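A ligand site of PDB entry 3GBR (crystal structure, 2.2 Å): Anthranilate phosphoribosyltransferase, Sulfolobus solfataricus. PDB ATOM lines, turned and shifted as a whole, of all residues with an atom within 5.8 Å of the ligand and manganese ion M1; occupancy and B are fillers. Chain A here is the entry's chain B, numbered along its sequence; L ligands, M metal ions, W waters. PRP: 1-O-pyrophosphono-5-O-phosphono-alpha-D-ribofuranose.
The backbone NH of Ser 118 sits at hydrogen-bond distance from an oxygen (O2) of the ligand. An oxygen (O3B) of the ligand sits at hydrogen-bond distance from the side-chain hydroxyl of Thr 92. N of Thr 92 lies within hydrogen-bond range of O3B of the ligand, 2.8 Å away. NZ of Lys 106 is in salt-bridge range of O1A of the ligand. ND2 of Asn 89 sits at hydrogen-bond distance from O2B of the ligand (2.8 Å). An oxygen (O3B) of the ligand sits at hydrogen-bond distance from the backbone NH of Val 90 (3.5 Å). An oxygen (O3B) of the ligand is in hydrogen-bond range of the backbone NH of Ser 91 (3.3 Å). O2A of the ligand sits close to N of Gly 79 (2.9 Å).
The side-chain amide oxygen (OD1) of Asn 89 lies within hydrogen-bond range of the side-chain hydroxyl (OG) of Ser 116 (2.6 Å). The backbone carbonyl oxygen of Thr 77 sits at hydrogen-bond distance from the side-chain amino group of Lys 106 (3.0 Å). The side-chain carboxylate (OD2) of Asp 223 is in hydrogen-bond range of the backbone NH (N) of Thr 80, at 3.4 Å. The side-chain carboxylate of Asp 223 sits at hydrogen-bond distance from the backbone NH of Gly 81 (2.7 Å). OG1 of Thr 92 is in hydrogen-bond range of OG of Ser 118, at 2.8 Å.
CA of Ala 78 touches O2A of the ligand, at 3.3 Å. Thr 80 touches the ligand (O to C5, 3.4 Å). N of Gly 81 touches C4 of the ligand (3.7 Å). Gly 117 touches the ligand. 12 residues have an atom within 4 Å of the ligand: Ala 78, Gly 79, Thr 80, Gly 81, Asn 89, Val 90, Ser 91, Thr 92, Lys 106, Gly 117, Ser 118 and Glu 224. Along chain A the residues within 4 Å of the ligand span positions 78 to 224. The nearest printed residue that does not touch the ligand is Thr 77 (4.2 Å).
N of Gly 79 touches manganese ion M1 (3.96 Å). Three residues have an atom within 4 Å of manganese ion M1: Gly 79, Ser 91 and Glu 224. Along chain A the residues within 4 Å of manganese ion M1 span positions 79 to 224.
Manganese ion M1 is bound by an oxygen (O1B) of the ligand (1.9 Å), the side-chain carboxylate of Glu 224 (2.0 Å), an oxygen (O2A) of the ligand (2.1 Å), water W3 (2.2 Å), the side-chain hydroxyl of Ser 91 (2.3 Å) and water W7 (2.5 Å). Manganese ion M1 has six donor atoms within binding distance.
Water W3 lies within hydrogen-bond range of the backbone carbonyl oxygen (O) of Asp 223 (2.8 Å), the backbone NH (N) of Gly 79 (3.0 Å) and the side-chain carboxylate (OE2) of Glu 224 (3.1 Å). Water W7 lies within hydrogen-bond range of the side-chain carboxylate (OD2) of Asp 223 (2.7 Å) and an oxygen (O1) of the ligand (2.9 Å). Water W9 lies within hydrogen-bond range of an oxygen (O1P) of the ligand (2.7 Å), the side-chain amide oxygen of Asn 174 (2.9 Å) and the backbone carbonyl oxygen of Thr 80 (3.0 Å). Water W6 lies within hydrogen-bond range of O of His 107 (2.6 Å) and O1A of the ligand (2.9 Å). Water W4 lies within hydrogen-bond range of O of Asn 109 (2.9 Å), O3P of the ligand (3.0 Å) and N of Ala 111 (3.5 Å). Water W8 lies within hydrogen-bond range of O of Gly 79 (3.1 Å) and O4 of the ligand (3.3 Å).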
ATOM      1  N   THR A  77     -29.097  16.019  -3.659  1.00  0.00           N
ATOM      2  CA  THR A  77     -27.820  15.492  -3.216  1.00  0.00           C
ATOM      3  C   THR A  77     -27.177  16.572  -2.340  1.00  0.00           C
ATOM      4  O   THR A  77     -26.843  17.649  -2.823  1.00  0.00           O
ATOM      5  CB  THR A  77     -26.905  15.099  -4.394  1.00  0.00           C
ATOM      6  OG1 THR A  77     -25.605  14.761  -3.891  1.00  0.00           O
ATOM      7  CG2 THR A  77     -26.791  16.239  -5.419  1.00  0.00           C
ATOM      8  N   ALA A  78     -27.055  16.274  -1.052  1.00  0.00           N
ATOM      9  CA  ALA A  78     -26.640  17.280  -0.063  1.00  0.00           C
ATOM     10  C   ALA A  78     -26.046  16.591   1.151  1.00  0.00           C
ATOM     11  O   ALA A  78     -26.440  15.476   1.494  1.00  0.00           O
ATOM     12  CB  ALA A  78     -27.813  18.158   0.362  1.00  0.00           C
ATOM     13  N   GLY A  79     -25.098  17.253   1.807  1.00  0.00           N
ATOM     14  CA  GLY A  79     -24.427  16.679   2.959  1.00  0.00           C
ATOM     15  C   GLY A  79     -24.564  17.524   4.202  1.00  0.00           C
ATOM     16  O   GLY A  79     -25.032  18.658   4.148  1.00  0.00           O
ATOM     17  N   THR A  80     -24.157  16.957   5.335  1.00  0.00           N
ATOM     18  CA  THR A  80     -24.223  17.642   6.617  1.00  0.00           C
ATOM     19  C   THR A  80     -23.137  18.693   6.765  1.00  0.00           C
ATOM     20  O   THR A  80     -23.257  19.571   7.618  1.00  0.00           O
ATOM     21  CB  THR A  80     -24.060  16.663   7.800  1.00  0.00           C
ATOM     22  OG1 THR A  80     -22.809  15.980   7.678  1.00  0.00           O
ATOM     23  CG2 THR A  80     -25.216  15.664   7.844  1.00  0.00           C
ATOM     24  N   GLY A  81     -22.097  18.605   5.947  1.00  0.00           N
ATOM     25  CA  GLY A  81     -20.878  19.389   6.144  1.00  0.00           C
ATOM     26  C   GLY A  81     -20.183  18.895   7.403  1.00  0.00           C
ATOM     27  O   GLY A  81     -20.603  17.906   7.980  1.00  0.00           O
ATOM     28  N   GLY A  82     -19.112  19.573   7.797  1.00  0.00           N
ATOM     29  CA  GLY A  82     -18.420  19.259   9.063  1.00  0.00           C
ATOM     30  C   GLY A  82     -17.000  18.734   8.926  1.00  0.00           C
ATOM     31  O   GLY A  82     -16.209  18.834   9.868  1.00  0.00           O
ATOM     32  N   VAL A  88     -13.892  20.915  -3.419  1.00  0.00           N
ATOM     33  CA  VAL A  88     -14.815  21.468  -4.411  1.00  0.00           C
ATOM     34  C   VAL A  88     -16.274  21.142  -4.055  1.00  0.00           C
ATOM     35  O   VAL A  88     -16.561  20.113  -3.449  1.00  0.00           O
ATOM     36  CB  VAL A  88     -14.471  20.939  -5.824  1.00  0.00           C
ATOM     37  CG1 VAL A  88     -14.694  19.419  -5.894  1.00  0.00           C
ATOM     38  CG2 VAL A  88     -15.266  21.666  -6.904  1.00  0.00           C
ATOM     39  N   ASN A  89     -17.189  22.036  -4.426  1.00  0.00           N
ATOM     40  CA  ASN A  89     -18.625  21.831  -4.153  1.00  0.00           C
ATOM     41  C   ASN A  89     -19.223  20.778  -5.085  1.00  0.00           C
ATOM     42  O   ASN A  89     -19.848  21.093  -6.104  1.00  0.00           O
ATOM     43  CB  ASN A  89     -19.372  23.158  -4.277  1.00  0.00           C
ATOM     44  CG  ASN A  89     -18.945  24.144  -3.229  1.00  0.00           C
ATOM     45  OD1 ASN A  89     -18.166  25.048  -3.507  1.00  0.00           O
ATOM     46  ND2 ASN A  89     -19.428  23.969  -2.017  1.00  0.00           N
ATOM     47  N   VAL A  90     -19.033  19.524  -4.724  1.00  0.00           N
ATOM     48  CA  VAL A  90     -19.269  18.417  -5.630  1.00  0.00           C
ATOM     49  C   VAL A  90     -20.761  18.056  -5.779  1.00  0.00           C
ATOM     50  O   VAL A  90     -21.182  17.708  -6.885  1.00  0.00           O
ATOM     51  CB  VAL A  90     -18.442  17.169  -5.220  1.00  0.00           C
ATOM     52  CG1 VAL A  90     -18.978  16.553  -3.940  1.00  0.00           C
ATOM     53  CG2 VAL A  90     -18.397  16.156  -6.352  1.00  0.00           C
ATOM     54  N   SER A  91     -21.539  18.122  -4.701  1.00  0.00           N
ATOM     55  CA  SER A  91     -22.990  17.870  -4.800  1.00  0.00           C
ATOM     56  C   SER A  91     -23.694  18.909  -5.692  1.00  0.00           C
ATOM     57  O   SER A  91     -24.663  18.577  -6.385  1.00  0.00           O
ATOM     58  CB  SER A  91     -23.631  17.866  -3.413  1.00  0.00           C
ATOM     59  OG  SER A  91     -22.954  16.998  -2.509  1.00  0.00           O
ATOM     60  N   THR A  92     -23.229  20.153  -5.673  1.00  0.00           N
ATOM     61  CA  THR A  92     -23.785  21.203  -6.531  1.00  0.00           C
ATOM     62  C   THR A  92     -23.548  20.890  -8.018  1.00  0.00           C
ATOM     63  O   THR A  92     -24.473  20.978  -8.834  1.00  0.00           O
ATOM     64  CB  THR A  92     -23.202  22.593  -6.181  1.00  0.00           C
ATOM     65  OG1 THR A  92     -23.433  22.880  -4.798  1.00  0.00           O
ATOM     66  CG2 THR A  92     -23.826  23.686  -7.044  1.00  0.00           C
ATOM     67  N   ALA A  93     -22.312  20.552  -8.356  1.00  0.00           N
ATOM     68  CA  ALA A  93     -21.955  20.068  -9.698  1.00  0.00           C
ATOM     69  C   ALA A  93     -22.757  18.818 -10.079  1.00  0.00           C
ATOM     70  O   ALA A  93     -23.234  18.699 -11.198  1.00  0.00           O
ATOM     71  CB  ALA A  93     -20.456  19.775  -9.763  1.00  0.00           C
ATOM     72  N   LYS A 106     -32.218  21.508  -4.559  1.00  0.00           N
ATOM     73  CA  LYS A 106     -31.277  21.709  -3.447  1.00  0.00           C
ATOM     74  C   LYS A 106     -31.742  22.844  -2.544  1.00  0.00           C
ATOM     75  O   LYS A 106     -32.554  23.682  -2.936  1.00  0.00           O
ATOM     76  CB  LYS A 106     -29.881  22.057  -3.979  1.00  0.00           C
ATOM     77  CG  LYS A 106     -29.156  20.920  -4.689  1.00  0.00           C
ATOM     78  CD  LYS A 106     -27.707  21.323  -4.935  1.00  0.00           C
ATOM     79  CE  LYS A 106     -26.750  20.772  -3.893  1.00  0.00           C
ATOM     80  NZ  LYS A 106     -27.324  20.642  -2.536  1.00  0.00           N
ATOM     81  N   HIS A 107     -31.202  22.881  -1.328  1.00  0.00           N
ATOM     82  CA  HIS A 107     -31.444  23.996  -0.422  1.00  0.00           C
ATOM     83  C   HIS A 107     -30.236  24.261   0.469  1.00  0.00           C
ATOM     84  O   HIS A 107     -29.399  23.377   0.691  1.00  0.00           O
ATOM     85  CB  HIS A 107     -32.673  23.719   0.443  1.00  0.00           C
ATOM     86  CG  HIS A 107     -32.491  22.587   1.404  1.00  0.00           C
ATOM     87  ND1 HIS A 107     -32.591  22.755   2.768  1.00  0.00           N
ATOM     88  CD2 HIS A 107     -32.209  21.281   1.200  1.00  0.00           C
ATOM     89  CE1 HIS A 107     -32.377  21.582   3.369  1.00  0.00           C
ATOM     90  NE2 HIS A 107     -32.152  20.683   2.432  1.00  0.00           N
ATOM     91  N   ASN A 109     -27.766  27.569   2.808  1.00  0.00           N
ATOM     92  CA  ASN A 109     -27.364  28.921   3.172  1.00  0.00           C
ATOM     93  C   ASN A 109     -26.062  29.286   2.504  1.00  0.00           C
ATOM     94  O   ASN A 109     -25.246  28.416   2.202  1.00  0.00           O
ATOM     95  CB  ASN A 109     -27.129  28.982   4.674  1.00  0.00           C
ATOM     96  CG  ASN A 109     -28.402  28.872   5.476  1.00  0.00           C
ATOM     97  OD1 ASN A 109     -29.168  29.837   5.572  1.00  0.00           O
ATOM     98  ND2 ASN A 109     -28.630  27.706   6.086  1.00  0.00           N
ATOM     99  N   ARG A 110     -25.845  30.583   2.335  1.00  0.00           N
ATOM    100  CA  ARG A 110     -24.502  31.076   2.094  1.00  0.00           C
ATOM    101  C   ARG A 110     -23.602  30.604   3.246  1.00  0.00           C
ATOM    102  O   ARG A 110     -24.038  30.563   4.392  1.00  0.00           O
ATOM    103  CB  ARG A 110     -24.470  32.597   2.034  1.00  0.00           C
ATOM    104  CG  ARG A 110     -25.104  33.209   0.816  1.00  0.00           C
ATOM    105  CD  ARG A 110     -24.545  34.597   0.583  1.00  0.00           C
ATOM    106  NE  ARG A 110     -25.234  35.314  -0.491  1.00  0.00           N
ATOM    107  CZ  ARG A 110     -26.368  35.996  -0.362  1.00  0.00           C
ATOM    108  NH1 ARG A 110     -26.877  36.613  -1.407  1.00  0.00           N
ATOM    109  NH2 ARG A 110     -26.998  36.059   0.806  1.00  0.00           N
ATOM    110  N   ALA A 111     -22.374  30.238   2.920  1.00  0.00           N
ATOM    111  CA  ALA A 111     -21.375  29.838   3.936  1.00  0.00           C
ATOM    112  C   ALA A 111     -20.882  31.061   4.698  1.00  0.00           C
ATOM    113  O   ALA A 111     -21.068  32.199   4.264  1.00  0.00           O
ATOM    114  CB  ALA A 111     -20.203  29.131   3.266  1.00  0.00           C
ATOM    115  N   SER A 116     -16.863  28.223   1.024  1.00  0.00           N
ATOM    116  CA  SER A 116     -17.697  28.060  -0.171  1.00  0.00           C
ATOM    117  C   SER A 116     -18.796  27.006   0.021  1.00  0.00           C
ATOM    118  O   SER A 116     -18.518  25.786   0.001  1.00  0.00           O
ATOM    119  CB  SER A 116     -16.848  27.664  -1.373  1.00  0.00           C
ATOM    120  OG  SER A 116     -17.654  27.438  -2.512  1.00  0.00           O
ATOM    121  N   GLY A 117     -20.023  27.483   0.192  1.00  0.00           N
ATOM    122  CA  GLY A 117     -21.184  26.597   0.231  1.00  0.00           C
ATOM    123  C   GLY A 117     -21.784  26.427  -1.157  1.00  0.00           C
ATOM    124  O   GLY A 117     -21.343  27.044  -2.109  1.00  0.00           O
ATOM    125  N   SER A 118     -22.797  25.575  -1.260  1.00  0.00           N
ATOM    126  CA  SER A 118     -23.532  25.406  -2.523  1.00  0.00           C
ATOM    127  C   SER A 118     -24.119  26.723  -3.042  1.00  0.00           C
ATOM    128  O   SER A 118     -24.035  27.010  -4.236  1.00  0.00           O
ATOM    129  CB  SER A 118     -24.663  24.384  -2.337  1.00  0.00           C
ATOM    130  OG  SER A 118     -25.450  24.284  -3.518  1.00  0.00           O
ATOM    131  N   ALA A 119     -24.699  27.517  -2.145  1.00  0.00           N
ATOM    132  CA  ALA A 119     -25.284  28.816  -2.517  1.00  0.00           C
ATOM    133  C   ALA A 119     -24.230  29.722  -3.128  1.00  0.00           C
ATOM    134  O   ALA A 119     -24.496  30.390  -4.135  1.00  0.00           O
ATOM    135  CB  ALA A 119     -25.908  29.493  -1.309  1.00  0.00           C
ATOM    136  N   VAL A 121     -21.235  28.965  -4.602  1.00  0.00           N
ATOM    137  CA  VAL A 121     -20.734  28.552  -5.893  1.00  0.00           C
ATOM    138  C   VAL A 121     -21.783  28.819  -6.958  1.00  0.00           C
ATOM    139  O   VAL A 121     -21.454  29.257  -8.057  1.00  0.00           O
ATOM    140  CB  VAL A 121     -20.290  27.066  -5.945  1.00  0.00           C
ATOM    141  CG1 VAL A 121     -21.467  26.131  -5.948  1.00  0.00           C
ATOM    142  CG2 VAL A 121     -19.451  26.831  -7.171  1.00  0.00           C
ATOM    143  N   ASN A 174     -26.823  20.600  12.956  1.00  0.00           N
ATOM    144  CA  ASN A 174     -25.806  20.443  11.934  1.00  0.00           C
ATOM    145  C   ASN A 174     -25.842  19.100  11.213  1.00  0.00           C
ATOM    146  O   ASN A 174     -25.086  18.884  10.275  1.00  0.00           O
ATOM    147  CB  ASN A 174     -24.425  20.663  12.546  1.00  0.00           C
ATOM    148  CG  ASN A 174     -24.163  22.111  12.875  1.00  0.00           C
ATOM    149  OD1 ASN A 174     -24.098  22.954  11.978  1.00  0.00           O
ATOM    150  ND2 ASN A 174     -24.026  22.407  14.147  1.00  0.00           N
ATOM    151  N   ASP A 223     -18.283  14.247   3.897  1.00  0.00           N
ATOM    152  CA  ASP A 223     -19.702  14.017   3.648  1.00  0.00           C
ATOM    153  C   ASP A 223     -19.988  13.871   2.140  1.00  0.00           C
ATOM    154  O   ASP A 223     -20.831  14.570   1.578  1.00  0.00           O
ATOM    155  CB  ASP A 223     -20.544  15.144   4.261  1.00  0.00           C
ATOM    156  CG  ASP A 223     -20.271  16.500   3.639  1.00  0.00           C
ATOM    157  OD1 ASP A 223     -19.147  16.698   3.101  1.00  0.00           O
ATOM    158  OD2 ASP A 223     -21.177  17.366   3.688  1.00  0.00           O
ATOM    159  N   GLU A 224     -19.248  12.952   1.503  1.00  0.00           N
ATOM    160  CA  GLU A 224     -19.350  12.704   0.061  1.00  0.00           C
ATOM    161  C   GLU A 224     -18.854  11.290  -0.206  1.00  0.00           C
ATOM    162  O   GLU A 224     -18.325  10.628   0.686  1.00  0.00           O
ATOM    163  CB  GLU A 224     -18.475  13.660  -0.755  1.00  0.00           C
ATOM    164  CG  GLU A 224     -18.703  15.160  -0.530  1.00  0.00           C
ATOM    165  CD  GLU A 224     -20.048  15.664  -1.043  1.00  0.00           C
ATOM    166  OE1 GLU A 224     -20.378  16.819  -0.743  1.00  0.00           O
ATOM    167  OE2 GLU A 224     -20.760  14.920  -1.748  1.00  0.00           O
HETATM  168  C1  PRP L   1     -23.848  21.986   1.790  1.00  0.00           C
HETATM  169  C2  PRP L   1     -22.705  22.899   2.050  1.00  0.00           C
HETATM  170  C3  PRP L   1     -22.020  22.403   3.240  1.00  0.00           C
HETATM  171  C4  PRP L   1     -23.064  21.505   3.908  1.00  0.00           C
HETATM  172  C5  PRP L   1     -23.547  22.019   5.255  1.00  0.00           C
HETATM  173  O1  PRP L   1     -23.324  20.933   0.992  1.00  0.00           O
HETATM  174  O2  PRP L   1     -22.259  23.590   0.882  1.00  0.00           O
HETATM  175  O3  PRP L   1     -20.941  21.601   2.759  1.00  0.00           O
HETATM  176  O4  PRP L   1     -24.204  21.414   3.044  1.00  0.00           O
HETATM  177  O5  PRP L   1     -24.066  23.342   5.139  1.00  0.00           O
HETATM  178  P   PRP L   1     -24.011  24.385   6.380  1.00  0.00           P
HETATM  179  O1P PRP L   1     -24.905  23.768   7.418  1.00  0.00           O
HETATM  180  O2P PRP L   1     -22.536  24.379   6.763  1.00  0.00           O
HETATM  181  O3P PRP L   1     -24.480  25.692   5.805  1.00  0.00           O
HETATM  182  PA  PRP L   1     -24.057  20.396  -0.302  1.00  0.00           P
HETATM  183  O1A PRP L   1     -25.476  20.888  -0.318  1.00  0.00           O
HETATM  184  O2A PRP L   1     -23.818  18.910  -0.237  1.00  0.00           O
HETATM  185  O3A PRP L   1     -23.284  21.060  -1.552  1.00  0.00           O
HETATM  186  PB  PRP L   1     -21.764  20.807  -2.012  1.00  0.00           P
HETATM  187  O1B PRP L   1     -21.422  19.343  -1.734  1.00  0.00           O
HETATM  188  O2B PRP L   1     -21.017  21.831  -1.210  1.00  0.00           O
HETATM  189  O3B PRP L   1     -21.803  21.202  -3.454  1.00  0.00           O
HETATM  190 MN    MN M   1     -22.023  17.902  -0.599  1.00  0.00          MN
HETATM  191 MN    MN M   2     -18.430  18.145   0.843  1.00  0.00          MN
HETATM  192  O   HOH W   1     -20.869  26.070   4.732  1.00  0.00           O
HETATM  193  O   HOH W   2     -21.164  22.675   8.050  1.00  0.00           O
HETATM  194  O   HOH W   3     -22.789  16.105   0.337  1.00  0.00           O
HETATM  195  O   HOH W   4     -23.111  26.855   3.380  1.00  0.00           O
HETATM  196  O   HOH W   5     -26.369  25.680   9.176  1.00  0.00           O
HETATM  197  O   HOH W   6     -26.772  23.393   0.403  1.00  0.00           O
HETATM  198  O   HOH W   7     -21.299  18.912   1.527  1.00  0.00           O
HETATM  199  O   HOH W   8     -27.320  20.762   3.972  1.00  0.00           O
HETATM  200  O   HOH W   9     -24.028  21.939   9.260  1.00  0.00           O
HETATM  201  O   HOH W  10     -18.892  20.785   0.332  1.00  0.00           O
